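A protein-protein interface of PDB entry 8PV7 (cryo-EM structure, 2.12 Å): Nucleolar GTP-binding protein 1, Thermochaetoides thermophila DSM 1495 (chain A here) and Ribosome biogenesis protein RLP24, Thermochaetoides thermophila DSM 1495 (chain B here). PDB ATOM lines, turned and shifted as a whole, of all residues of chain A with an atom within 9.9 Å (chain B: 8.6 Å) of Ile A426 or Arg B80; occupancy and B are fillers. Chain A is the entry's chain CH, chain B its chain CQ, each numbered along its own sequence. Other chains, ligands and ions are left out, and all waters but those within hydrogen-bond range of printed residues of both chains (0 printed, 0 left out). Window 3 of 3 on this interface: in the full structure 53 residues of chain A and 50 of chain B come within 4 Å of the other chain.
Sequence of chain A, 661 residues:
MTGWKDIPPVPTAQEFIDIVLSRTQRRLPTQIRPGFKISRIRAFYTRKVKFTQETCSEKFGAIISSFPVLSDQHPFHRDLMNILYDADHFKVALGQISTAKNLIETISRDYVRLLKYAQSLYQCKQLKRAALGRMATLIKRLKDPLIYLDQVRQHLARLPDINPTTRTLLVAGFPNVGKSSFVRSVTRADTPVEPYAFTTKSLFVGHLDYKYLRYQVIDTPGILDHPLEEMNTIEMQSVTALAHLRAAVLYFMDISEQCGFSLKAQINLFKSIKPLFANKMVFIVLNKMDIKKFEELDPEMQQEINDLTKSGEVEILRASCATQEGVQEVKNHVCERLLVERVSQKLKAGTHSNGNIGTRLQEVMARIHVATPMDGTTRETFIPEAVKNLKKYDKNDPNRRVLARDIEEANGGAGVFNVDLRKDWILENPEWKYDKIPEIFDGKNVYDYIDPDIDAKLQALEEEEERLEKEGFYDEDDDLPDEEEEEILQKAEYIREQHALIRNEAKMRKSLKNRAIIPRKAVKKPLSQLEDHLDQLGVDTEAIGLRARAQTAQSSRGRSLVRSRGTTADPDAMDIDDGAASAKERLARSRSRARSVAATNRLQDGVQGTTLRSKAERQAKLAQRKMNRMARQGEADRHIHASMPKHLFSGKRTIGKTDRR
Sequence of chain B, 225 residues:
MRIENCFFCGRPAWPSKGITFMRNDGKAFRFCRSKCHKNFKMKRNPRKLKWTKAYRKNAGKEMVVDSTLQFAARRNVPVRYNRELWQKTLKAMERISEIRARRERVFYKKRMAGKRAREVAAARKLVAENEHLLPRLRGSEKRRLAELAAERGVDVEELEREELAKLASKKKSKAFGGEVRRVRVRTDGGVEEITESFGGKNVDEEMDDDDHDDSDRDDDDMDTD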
ATOM      1  N   LEU A 421      -7.923  17.321  -5.434  1.00  0.00           N
ATOM      2  CA  LEU A 421      -7.966  18.541  -6.230  1.00  0.00           C
ATOM      3  C   LEU A 421      -8.030  19.810  -5.393  1.00  0.00           C
ATOM      4  O   LEU A 421      -7.745  20.889  -5.917  1.00  0.00           O
ATOM      5  CB  LEU A 421      -9.159  18.505  -7.186  1.00  0.00           C
ATOM      6  CG  LEU A 421      -9.170  17.426  -8.267  1.00  0.00           C
ATOM      7  CD1 LEU A 421     -10.464  17.482  -9.049  1.00  0.00           C
ATOM      8  CD2 LEU A 421      -7.980  17.580  -9.190  1.00  0.00           C
ATOM      9  N   ARG A 422      -8.389  19.714  -4.117  1.00  0.00           N
ATOM     10  CA  ARG A 422      -8.517  20.881  -3.256  1.00  0.00           C
ATOM     11  C   ARG A 422      -7.263  21.167  -2.450  1.00  0.00           C
ATOM     12  O   ARG A 422      -7.276  22.075  -1.619  1.00  0.00           O
ATOM     13  CB  ARG A 422      -9.703  20.706  -2.308  1.00  0.00           C
ATOM     14  CG  ARG A 422     -11.039  20.918  -2.972  1.00  0.00           C
ATOM     15  CD  ARG A 422     -12.108  20.147  -2.258  1.00  0.00           C
ATOM     16  NE  ARG A 422     -13.417  20.343  -2.861  1.00  0.00           N
ATOM     17  CZ  ARG A 422     -14.383  21.076  -2.331  1.00  0.00           C
ATOM     18  NH1 ARG A 422     -14.208  21.729  -1.196  1.00  0.00           N
ATOM     19  NH2 ARG A 422     -15.555  21.150  -2.953  1.00  0.00           N
ATOM     20  N   LYS A 423      -6.186  20.413  -2.673  1.00  0.00           N
ATOM     21  CA  LYS A 423      -4.973  20.585  -1.884  1.00  0.00           C
ATOM     22  C   LYS A 423      -4.295  21.918  -2.178  1.00  0.00           C
ATOM     23  O   LYS A 423      -3.712  22.537  -1.282  1.00  0.00           O
ATOM     24  CB  LYS A 423      -4.016  19.427  -2.154  1.00  0.00           C
ATOM     25  CG  LYS A 423      -2.836  19.348  -1.210  1.00  0.00           C
ATOM     26  CD  LYS A 423      -1.985  18.095  -1.432  1.00  0.00           C
ATOM     27  CE  LYS A 423      -1.197  18.121  -2.742  1.00  0.00           C
ATOM     28  NZ  LYS A 423      -1.950  17.655  -3.944  1.00  0.00           N
ATOM     29  N   ASP A 424      -4.362  22.378  -3.425  1.00  0.00           N
ATOM     30  CA  ASP A 424      -3.696  23.605  -3.831  1.00  0.00           C
ATOM     31  C   ASP A 424      -4.652  24.789  -3.937  1.00  0.00           C
ATOM     32  O   ASP A 424      -4.335  25.771  -4.612  1.00  0.00           O
ATOM     33  CB  ASP A 424      -2.962  23.389  -5.152  1.00  0.00           C
ATOM     34  CG  ASP A 424      -1.779  22.453  -5.011  1.00  0.00           C
ATOM     35  OD1 ASP A 424      -1.455  22.070  -3.868  1.00  0.00           O
ATOM     36  OD2 ASP A 424      -1.171  22.101  -6.041  1.00  0.00           O
ATOM     37  N   TRP A 425      -5.812  24.713  -3.290  1.00  0.00           N
ATOM     38  CA  TRP A 425      -6.708  25.857  -3.228  1.00  0.00           C
ATOM     39  C   TRP A 425      -6.120  26.937  -2.329  1.00  0.00           C
ATOM     40  O   TRP A 425      -5.604  26.653  -1.245  1.00  0.00           O
ATOM     41  CB  TRP A 425      -8.078  25.436  -2.701  1.00  0.00           C
ATOM     42  CG  TRP A 425      -9.014  24.941  -3.753  1.00  0.00           C
ATOM     43  CD1 TRP A 425      -8.708  24.628  -5.041  1.00  0.00           C
ATOM     44  CD2 TRP A 425     -10.417  24.701  -3.605  1.00  0.00           C
ATOM     45  NE1 TRP A 425      -9.829  24.208  -5.706  1.00  0.00           N
ATOM     46  CE2 TRP A 425     -10.894  24.244  -4.846  1.00  0.00           C
ATOM     47  CE3 TRP A 425     -11.317  24.832  -2.544  1.00  0.00           C
ATOM     48  CZ2 TRP A 425     -12.230  23.912  -5.055  1.00  0.00           C
ATOM     49  CZ3 TRP A 425     -12.639  24.501  -2.753  1.00  0.00           C
ATOM     50  CH2 TRP A 425     -13.085  24.050  -3.999  1.00  0.00           C
ATOM     51  N   ILE A 426      -6.192  28.181  -2.784  1.00  0.00           N
ATOM     52  CA  ILE A 426      -5.720  29.328  -2.019  1.00  0.00           C
ATOM     53  C   ILE A 426      -6.947  30.084  -1.535  1.00  0.00           C
ATOM     54  O   ILE A 426      -7.581  30.814  -2.304  1.00  0.00           O
ATOM     55  CB  ILE A 426      -4.804  30.237  -2.847  1.00  0.00           C
ATOM     56  CG1 ILE A 426      -3.922  29.410  -3.780  1.00  0.00           C
ATOM     57  CG2 ILE A 426      -3.951  31.091  -1.936  1.00  0.00           C
ATOM     58  CD1 ILE A 426      -3.296  30.224  -4.887  1.00  0.00           C
ATOM     59  N   LEU A 427      -7.285  29.911  -0.265  1.00  0.00           N
ATOM     60  CA  LEU A 427      -8.441  30.560   0.324  1.00  0.00           C
ATOM     61  C   LEU A 427      -7.995  31.518   1.418  1.00  0.00           C
ATOM     62  O   LEU A 427      -6.853  31.478   1.881  1.00  0.00           O
ATOM     63  CB  LEU A 427      -9.429  29.540   0.900  1.00  0.00           C
ATOM     64  CG  LEU A 427      -9.964  28.458  -0.038  1.00  0.00           C
ATOM     65  CD1 LEU A 427     -10.946  27.577   0.703  1.00  0.00           C
ATOM     66  CD2 LEU A 427     -10.614  29.067  -1.266  1.00  0.00           C
ATOM     67  N   GLU A 428      -8.918  32.396   1.814  1.00  0.00           N
ATOM     68  CA  GLU A 428      -8.641  33.317   2.909  1.00  0.00           C
ATOM     69  C   GLU A 428      -8.490  32.571   4.230  1.00  0.00           C
ATOM     70  O   GLU A 428      -7.660  32.942   5.067  1.00  0.00           O
ATOM     71  CB  GLU A 428      -9.740  34.380   3.001  1.00  0.00           C
ATOM     72  CG  GLU A 428     -10.125  35.047   1.671  1.00  0.00           C
ATOM     73  CD  GLU A 428     -11.198  34.303   0.877  1.00  0.00           C
ATOM     74  OE1 GLU A 428     -11.100  33.065   0.728  1.00  0.00           O
ATOM     75  OE2 GLU A 428     -12.141  34.968   0.396  1.00  0.00           O
ATOM     76  N   ASN A 429      -9.278  31.520   4.433  1.00  0.00           N
ATOM     77  CA  ASN A 429      -9.156  30.657   5.601  1.00  0.00           C
ATOM     78  C   ASN A 429      -8.867  29.236   5.135  1.00  0.00           C
ATOM     79  O   ASN A 429      -9.691  28.650   4.412  1.00  0.00           O
ATOM     80  CB  ASN A 429     -10.428  30.696   6.449  1.00  0.00           C
ATOM     81  CG  ASN A 429     -10.272  29.976   7.774  1.00  0.00           C
ATOM     82  OD1 ASN A 429      -9.166  29.632   8.179  1.00  0.00           O
ATOM     83  ND2 ASN A 429     -11.384  29.750   8.457  1.00  0.00           N
ATOM     84  N   PRO A 430      -7.730  28.643   5.510  1.00  0.00           N
ATOM     85  CA  PRO A 430      -7.420  27.279   5.045  1.00  0.00           C
ATOM     86  C   PRO A 430      -8.322  26.202   5.620  1.00  0.00           C
ATOM     87  O   PRO A 430      -8.304  25.073   5.118  1.00  0.00           O
ATOM     88  CB  PRO A 430      -5.965  27.079   5.492  1.00  0.00           C
ATOM     89  CG  PRO A 430      -5.433  28.456   5.685  1.00  0.00           C
ATOM     90  CD  PRO A 430      -6.583  29.260   6.192  1.00  0.00           C
ATOM     91  N   GLU A 431      -9.102  26.502   6.659  1.00  0.00           N
ATOM     92  CA  GLU A 431     -10.035  25.529   7.211  1.00  0.00           C
ATOM     93  C   GLU A 431     -11.243  25.291   6.313  1.00  0.00           C
ATOM     94  O   GLU A 431     -12.000  24.349   6.564  1.00  0.00           O
ATOM     95  CB  GLU A 431     -10.508  25.981   8.592  1.00  0.00           C
ATOM     96  CG  GLU A 431      -9.807  25.294   9.750  1.00  0.00           C
ATOM     97  CD  GLU A 431      -9.751  23.786   9.597  1.00  0.00           C
ATOM     98  OE1 GLU A 431     -10.809  23.133   9.717  1.00  0.00           O
ATOM     99  OE2 GLU A 431      -8.646  23.251   9.362  1.00  0.00           O
ATOM    100  N   TRP A 432     -11.442  26.117   5.287  1.00  0.00           N
ATOM    101  CA  TRP A 432     -12.569  25.992   4.376  1.00  0.00           C
ATOM    102  C   TRP A 432     -12.260  25.151   3.149  1.00  0.00           C
ATOM    103  O   TRP A 432     -13.119  25.032   2.273  1.00  0.00           O
ATOM    104  CB  TRP A 432     -13.032  27.373   3.906  1.00  0.00           C
ATOM    105  CG  TRP A 432     -13.428  28.320   4.977  1.00  0.00           C
ATOM    106  CD1 TRP A 432     -13.813  28.017   6.245  1.00  0.00           C
ATOM    107  CD2 TRP A 432     -13.489  29.743   4.866  1.00  0.00           C
ATOM    108  NE1 TRP A 432     -14.111  29.163   6.934  1.00  0.00           N
ATOM    109  CE2 TRP A 432     -13.920  30.239   6.108  1.00  0.00           C
ATOM    110  CE3 TRP A 432     -13.223  30.646   3.834  1.00  0.00           C
ATOM    111  CZ2 TRP A 432     -14.088  31.597   6.348  1.00  0.00           C
ATOM    112  CZ3 TRP A 432     -13.388  31.992   4.075  1.00  0.00           C
ATOM    113  CH2 TRP A 432     -13.816  32.455   5.322  1.00  0.00           C
ATOM    114  N   LYS A 433     -11.061  24.576   3.054  1.00  0.00           N
ATOM    115  CA  LYS A 433     -10.640  23.951   1.804  1.00  0.00           C
ATOM    116  C   LYS A 433     -11.386  22.661   1.503  1.00  0.00           C
ATOM    117  O   LYS A 433     -11.418  22.238   0.345  1.00  0.00           O
ATOM    118  CB  LYS A 433      -9.135  23.686   1.831  1.00  0.00           C
ATOM    119  CG  LYS A 433      -8.302  24.928   1.573  1.00  0.00           C
ATOM    120  CD  LYS A 433      -6.812  24.696   1.782  1.00  0.00           C
ATOM    121  CE  LYS A 433      -6.350  23.367   1.223  1.00  0.00           C
ATOM    122  NZ  LYS A 433      -4.892  23.181   1.417  1.00  0.00           N
ATOM    123  N   ILE A 437     -19.536  22.800  -0.901  1.00  0.00           N
ATOM    124  CA  ILE A 437     -20.031  24.089  -1.376  1.00  0.00           C
ATOM    125  C   ILE A 437     -21.465  23.942  -1.870  1.00  0.00           C
ATOM    126  O   ILE A 437     -21.725  23.131  -2.768  1.00  0.00           O
ATOM    127  CB  ILE A 437     -19.114  24.649  -2.472  1.00  0.00           C
ATOM    128  CG1 ILE A 437     -17.687  24.777  -1.936  1.00  0.00           C
ATOM    129  CG2 ILE A 437     -19.638  25.977  -2.973  1.00  0.00           C
ATOM    130  CD1 ILE A 437     -16.679  25.208  -2.960  1.00  0.00           C
ATOM    131  N   TYR A 447     -25.034  29.646  -7.174  1.00  0.00           N
ATOM    132  CA  TYR A 447     -24.026  30.358  -7.949  1.00  0.00           C
ATOM    133  C   TYR A 447     -24.629  31.504  -8.746  1.00  0.00           C
ATOM    134  O   TYR A 447     -23.928  32.469  -9.063  1.00  0.00           O
ATOM    135  CB  TYR A 447     -23.298  29.389  -8.877  1.00  0.00           C
ATOM    136  CG  TYR A 447     -22.187  28.625  -8.199  1.00  0.00           C
ATOM    137  CD1 TYR A 447     -22.467  27.568  -7.347  1.00  0.00           C
ATOM    138  CD2 TYR A 447     -20.860  28.969  -8.405  1.00  0.00           C
ATOM    139  CE1 TYR A 447     -21.458  26.870  -6.724  1.00  0.00           C
ATOM    140  CE2 TYR A 447     -19.844  28.274  -7.788  1.00  0.00           C
ATOM    141  CZ  TYR A 447     -20.148  27.226  -6.948  1.00  0.00           C
ATOM    142  OH  TYR A 447     -19.136  26.533  -6.330  1.00  0.00           O
ATOM    143  N   ILE A 450     -24.599  34.270  -6.056  1.00  0.00           N
ATOM    144  CA  ILE A 450     -23.327  34.676  -5.459  1.00  0.00           C
ATOM    145  C   ILE A 450     -22.915  36.030  -6.021  1.00  0.00           C
ATOM    146  O   ILE A 450     -22.787  36.206  -7.238  1.00  0.00           O
ATOM    147  CB  ILE A 450     -22.250  33.615  -5.700  1.00  0.00           C
ATOM    148  CG1 ILE A 450     -22.478  32.414  -4.789  1.00  0.00           C
ATOM    149  CG2 ILE A 450     -20.865  34.187  -5.446  1.00  0.00           C
ATOM    150  CD1 ILE A 450     -22.329  32.740  -3.331  1.00  0.00           C
ATOM    151  N   ASP A 451     -22.711  36.998  -5.129  1.00  0.00           N
ATOM    152  CA  ASP A 451     -22.384  38.356  -5.493  1.00  0.00           C
ATOM    153  C   ASP A 451     -21.561  38.921  -4.343  1.00  0.00           C
ATOM    154  O   ASP A 451     -22.001  38.827  -3.187  1.00  0.00           O
ATOM    155  CB  ASP A 451     -23.642  39.197  -5.718  1.00  0.00           C
ATOM    156  CG  ASP A 451     -23.340  40.580  -6.248  1.00  0.00           C
ATOM    157  OD1 ASP A 451     -22.421  40.717  -7.081  1.00  0.00           O
ATOM    158  OD2 ASP A 451     -24.024  41.537  -5.835  1.00  0.00           O
ATOM    159  N   PRO A 452     -20.367  39.458  -4.609  1.00  0.00           N
ATOM    160  CA  PRO A 452     -19.554  40.023  -3.515  1.00  0.00           C
ATOM    161  C   PRO A 452     -20.215  41.178  -2.777  1.00  0.00           C
ATOM    162  O   PRO A 452     -20.068  41.287  -1.554  1.00  0.00           O
ATOM    163  CB  PRO A 452     -18.270  40.469  -4.231  1.00  0.00           C
ATOM    164  CG  PRO A 452     -18.612  40.503  -5.686  1.00  0.00           C
ATOM    165  CD  PRO A 452     -19.642  39.449  -5.889  1.00  0.00           C
ATOM    166  N   VAL B  77     -17.867  36.030 -14.118  1.00  0.00           N
ATOM    167  CA  VAL B  77     -16.640  36.362 -13.398  1.00  0.00           C
ATOM    168  C   VAL B  77     -16.681  35.656 -12.050  1.00  0.00           C
ATOM    169  O   VAL B  77     -17.443  36.068 -11.165  1.00  0.00           O
ATOM    170  CB  VAL B  77     -16.480  37.881 -13.237  1.00  0.00           C
ATOM    171  CG1 VAL B  77     -15.190  38.208 -12.512  1.00  0.00           C
ATOM    172  CG2 VAL B  77     -16.518  38.556 -14.590  1.00  0.00           C
ATOM    173  N   PRO B  78     -15.908  34.589 -11.855  1.00  0.00           N
ATOM    174  CA  PRO B  78     -16.019  33.811 -10.617  1.00  0.00           C
ATOM    175  C   PRO B  78     -15.484  34.550  -9.399  1.00  0.00           C
ATOM    176  O   PRO B  78     -14.619  35.421  -9.493  1.00  0.00           O
ATOM    177  CB  PRO B  78     -15.189  32.558 -10.913  1.00  0.00           C
ATOM    178  CG  PRO B  78     -14.242  32.979 -11.956  1.00  0.00           C
ATOM    179  CD  PRO B  78     -14.974  33.969 -12.808  1.00  0.00           C
ATOM    180  N   VAL B  79     -16.017  34.174  -8.243  1.00  0.00           N
ATOM    181  CA  VAL B  79     -15.625  34.714  -6.950  1.00  0.00           C
ATOM    182  C   VAL B  79     -14.965  33.595  -6.158  1.00  0.00           C
ATOM    183  O   VAL B  79     -15.417  32.447  -6.205  1.00  0.00           O
ATOM    184  CB  VAL B  79     -16.847  35.293  -6.208  1.00  0.00           C
ATOM    185  CG1 VAL B  79     -16.473  35.810  -4.830  1.00  0.00           C
ATOM    186  CG2 VAL B  79     -17.484  36.395  -7.031  1.00  0.00           C
ATOM    187  N   ARG B  80     -13.864  33.921  -5.478  1.00  0.00           N
ATOM    188  CA  ARG B  80     -13.189  32.958  -4.616  1.00  0.00           C
ATOM    189  C   ARG B  80     -14.124  32.484  -3.512  1.00  0.00           C
ATOM    190  O   ARG B  80     -14.898  33.268  -2.958  1.00  0.00           O
ATOM    191  CB  ARG B  80     -11.937  33.586  -4.006  1.00  0.00           C
ATOM    192  CG  ARG B  80     -11.072  32.621  -3.213  1.00  0.00           C
ATOM    193  CD  ARG B  80      -9.751  33.252  -2.829  1.00  0.00           C
ATOM    194  NE  ARG B  80      -9.083  33.847  -3.978  1.00  0.00           N
ATOM    195  CZ  ARG B  80      -8.259  33.197  -4.786  1.00  0.00           C
ATOM    196  NH1 ARG B  80      -7.957  31.926  -4.589  1.00  0.00           N
ATOM    197  NH2 ARG B  80      -7.726  33.840  -5.819  1.00  0.00           N
ATOM    198  N   TYR B  81     -14.053  31.191  -3.200  1.00  0.00           N
ATOM    199  CA  TYR B  81     -14.990  30.598  -2.256  1.00  0.00           C
ATOM    200  C   TYR B  81     -14.778  31.148  -0.851  1.00  0.00           C
ATOM    201  O   TYR B  81     -13.648  31.228  -0.363  1.00  0.00           O
ATOM    202  CB  TYR B  81     -14.861  29.077  -2.237  1.00  0.00           C
ATOM    203  CG  TYR B  81     -15.639  28.451  -1.104  1.00  0.00           C
ATOM    204  CD1 TYR B  81     -17.026  28.514  -1.078  1.00  0.00           C
ATOM    205  CD2 TYR B  81     -14.993  27.827  -0.050  1.00  0.00           C
ATOM    206  CE1 TYR B  81     -17.743  27.965  -0.045  1.00  0.00           C
ATOM    207  CE2 TYR B  81     -15.704  27.270   0.988  1.00  0.00           C
ATOM    208  CZ  TYR B  81     -17.078  27.342   0.984  1.00  0.00           C
ATOM    209  OH  TYR B  81     -17.789  26.784   2.016  1.00  0.00           O
ATOM    210  N   ASN B  82     -15.881  31.515  -0.207  1.00  0.00           N
ATOM    211  CA  ASN B  82     -15.884  32.044   1.149  1.00  0.00           C
ATOM    212  C   ASN B  82     -17.109  31.482   1.849  1.00  0.00           C
ATOM    213  O   ASN B  82     -18.236  31.680   1.379  1.00  0.00           O
ATOM    214  CB  ASN B  82     -15.901  33.576   1.139  1.00  0.00           C
ATOM    215  CG  ASN B  82     -15.558  34.177   2.483  1.00  0.00           C
ATOM    216  OD1 ASN B  82     -16.172  33.859   3.499  1.00  0.00           O
ATOM    217  ND2 ASN B  82     -14.563  35.050   2.497  1.00  0.00           N
ATOM    218  N   ARG B  83     -16.882  30.784   2.966  1.00  0.00           N
ATOM    219  CA  ARG B  83     -17.963  30.082   3.653  1.00  0.00           C
ATOM    220  C   ARG B  83     -19.022  31.048   4.171  1.00  0.00           C
ATOM    221  O   ARG B  83     -20.226  30.797   4.021  1.00  0.00           O
ATOM    222  CB  ARG B  83     -17.392  29.247   4.798  1.00  0.00           C
ATOM    223  CG  ARG B  83     -18.445  28.520   5.612  1.00  0.00           C
ATOM    224  CD  ARG B  83     -17.869  27.936   6.879  1.00  0.00           C
ATOM    225  NE  ARG B  83     -16.978  26.813   6.624  1.00  0.00           N
ATOM    226  CZ  ARG B  83     -16.281  26.185   7.560  1.00  0.00           C
ATOM    227  NH1 ARG B  83     -16.325  26.569   8.825  1.00  0.00           N
ATOM    228  NH2 ARG B  83     -15.519  25.153   7.219  1.00  0.00           N
ATOM    229  N   LEU B  85     -19.683  34.070   3.038  1.00  0.00           N
ATOM    230  CA  LEU B  85     -20.378  34.644   1.894  1.00  0.00           C
ATOM    231  C   LEU B  85     -21.431  33.686   1.358  1.00  0.00           C
ATOM    232  O   LEU B  85     -22.548  34.105   1.036  1.00  0.00           O
ATOM    233  CB  LEU B  85     -19.376  35.017   0.801  1.00  0.00           C
ATOM    234  CG  LEU B  85     -19.979  35.463  -0.533  1.00  0.00           C
ATOM    235  CD1 LEU B  85     -20.779  36.737  -0.353  1.00  0.00           C
ATOM    236  CD2 LEU B  85     -18.910  35.651  -1.592  1.00  0.00           C
ATOM    237  N   TRP B  86     -21.110  32.392   1.298  1.00  0.00           N
ATOM    238  CA  TRP B  86     -22.084  31.413   0.818  1.00  0.00           C
ATOM    239  C   TRP B  86     -23.264  31.267   1.778  1.00  0.00           C
ATOM    240  O   TRP B  86     -24.417  31.156   1.336  1.00  0.00           O
ATOM    241  CB  TRP B  86     -21.401  30.067   0.581  1.00  0.00           C
ATOM    242  CG  TRP B  86     -21.206  29.745  -0.872  1.00  0.00           C
ATOM    243  CD1 TRP B  86     -21.899  28.831  -1.603  1.00  0.00           C
ATOM    244  CD2 TRP B  86     -20.254  30.332  -1.767  1.00  0.00           C
ATOM    245  NE1 TRP B  86     -21.446  28.812  -2.895  1.00  0.00           N
ATOM    246  CE2 TRP B  86     -20.435  29.723  -3.023  1.00  0.00           C
ATOM    247  CE3 TRP B  86     -19.271  31.314  -1.630  1.00  0.00           C
ATOM    248  CZ2 TRP B  86     -19.669  30.062  -4.132  1.00  0.00           C
ATOM    249  CZ3 TRP B  86     -18.513  31.649  -2.732  1.00  0.00           C
ATOM    250  CH2 TRP B  86     -18.715  31.025  -3.967  1.00  0.00           C
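The side-chain amide nitrogen (ND2) of Asn B82 is in hydrogen-bond range of the side-chain carboxylate (OE2) of Glu A428, 3.2 Å away.
The backbone carbonyl oxygen of Tyr B81 lies close to the side-chain carboxylate of Glu A428, 3.3 Å away.
NH1 of Arg B80 sits at hydrogen-bond distance from O of Ile A426 (2.6 Å).
The backbone NH (N) of Glu A431 sits close to the side-chain amide oxygen (OD1) of Asn A429, at 3.5 Å.
The side-chain amide nitrogen (ND2) of Asn A429 sits close to the indole nitrogen (NE1) of Trp A432 (3.2 Å).
Among the printed residues, pairs that only touch across the chains: Leu A427 with Tyr B81 (3.8 Å), Glu A428 with Arg B80 (3.8 Å), Glu A431 with Arg B83 (3.7 Å), Trp A432 with Tyr B81 (3.7 Å), Trp A432 with Asn B82 (3.3 Å), Trp A432 with Arg B83 (3.3 Å), Ile A437 with Tyr B81 (3.7 Å), Ile A437 with Trp B86 (3.4 Å), Ile A450 with Trp B86 (3.5 Å), Asp A451 with Leu B85 (3.7 Å) and Pro A452 with Val B79 (3.9 Å).
Of chain A, only Pro A452 (3.9 Å) comes within 4 Å of Val B79.
Printed residues of chain B within 4 Å of Glu A428: Arg B80, Tyr B81 and Asn B82.
Printed residues of chain A within 4 Å of Arg B83: Glu A431 (3.7 Å) and Trp A432 (3.3 Å).
Of the printed residues of chain B, Ile A450 touches Trp B86.
Printed residues of chain B within 4 Å of Pro A452: Val B79 (3.9 Å).
Of the printed residues of chain B, Glu A431 touches Arg B83.
Pro B78 touches none of the printed residues of chain A.
Asn A429 touches none of the printed residues of chain B.
The nearest printed residue of chain B that does not touch Ile A437 is Asn B82 (6.9 Å).
Of the 9 printed residues of chain B, 7 touch a printed residue of chain A.
Hydrophobic or aromatic side chains of chain B that line the printed part of chain A: Val B79, Tyr B81, Leu B85 and Trp B86.
Printed residues of chain A that touch a printed residue of chain B: Ile A426, Leu A427, Glu A428, Glu A431, Trp A432, Ile A437, Ile A450, Asp A451 and Pro A452.
Among the printed residues, 14 pairs touch across the chains.
Among the printed residues, no Asp or Glu carboxylate lies within 4 Å of a Lys or Arg side-chain nitrogen of the other chain.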
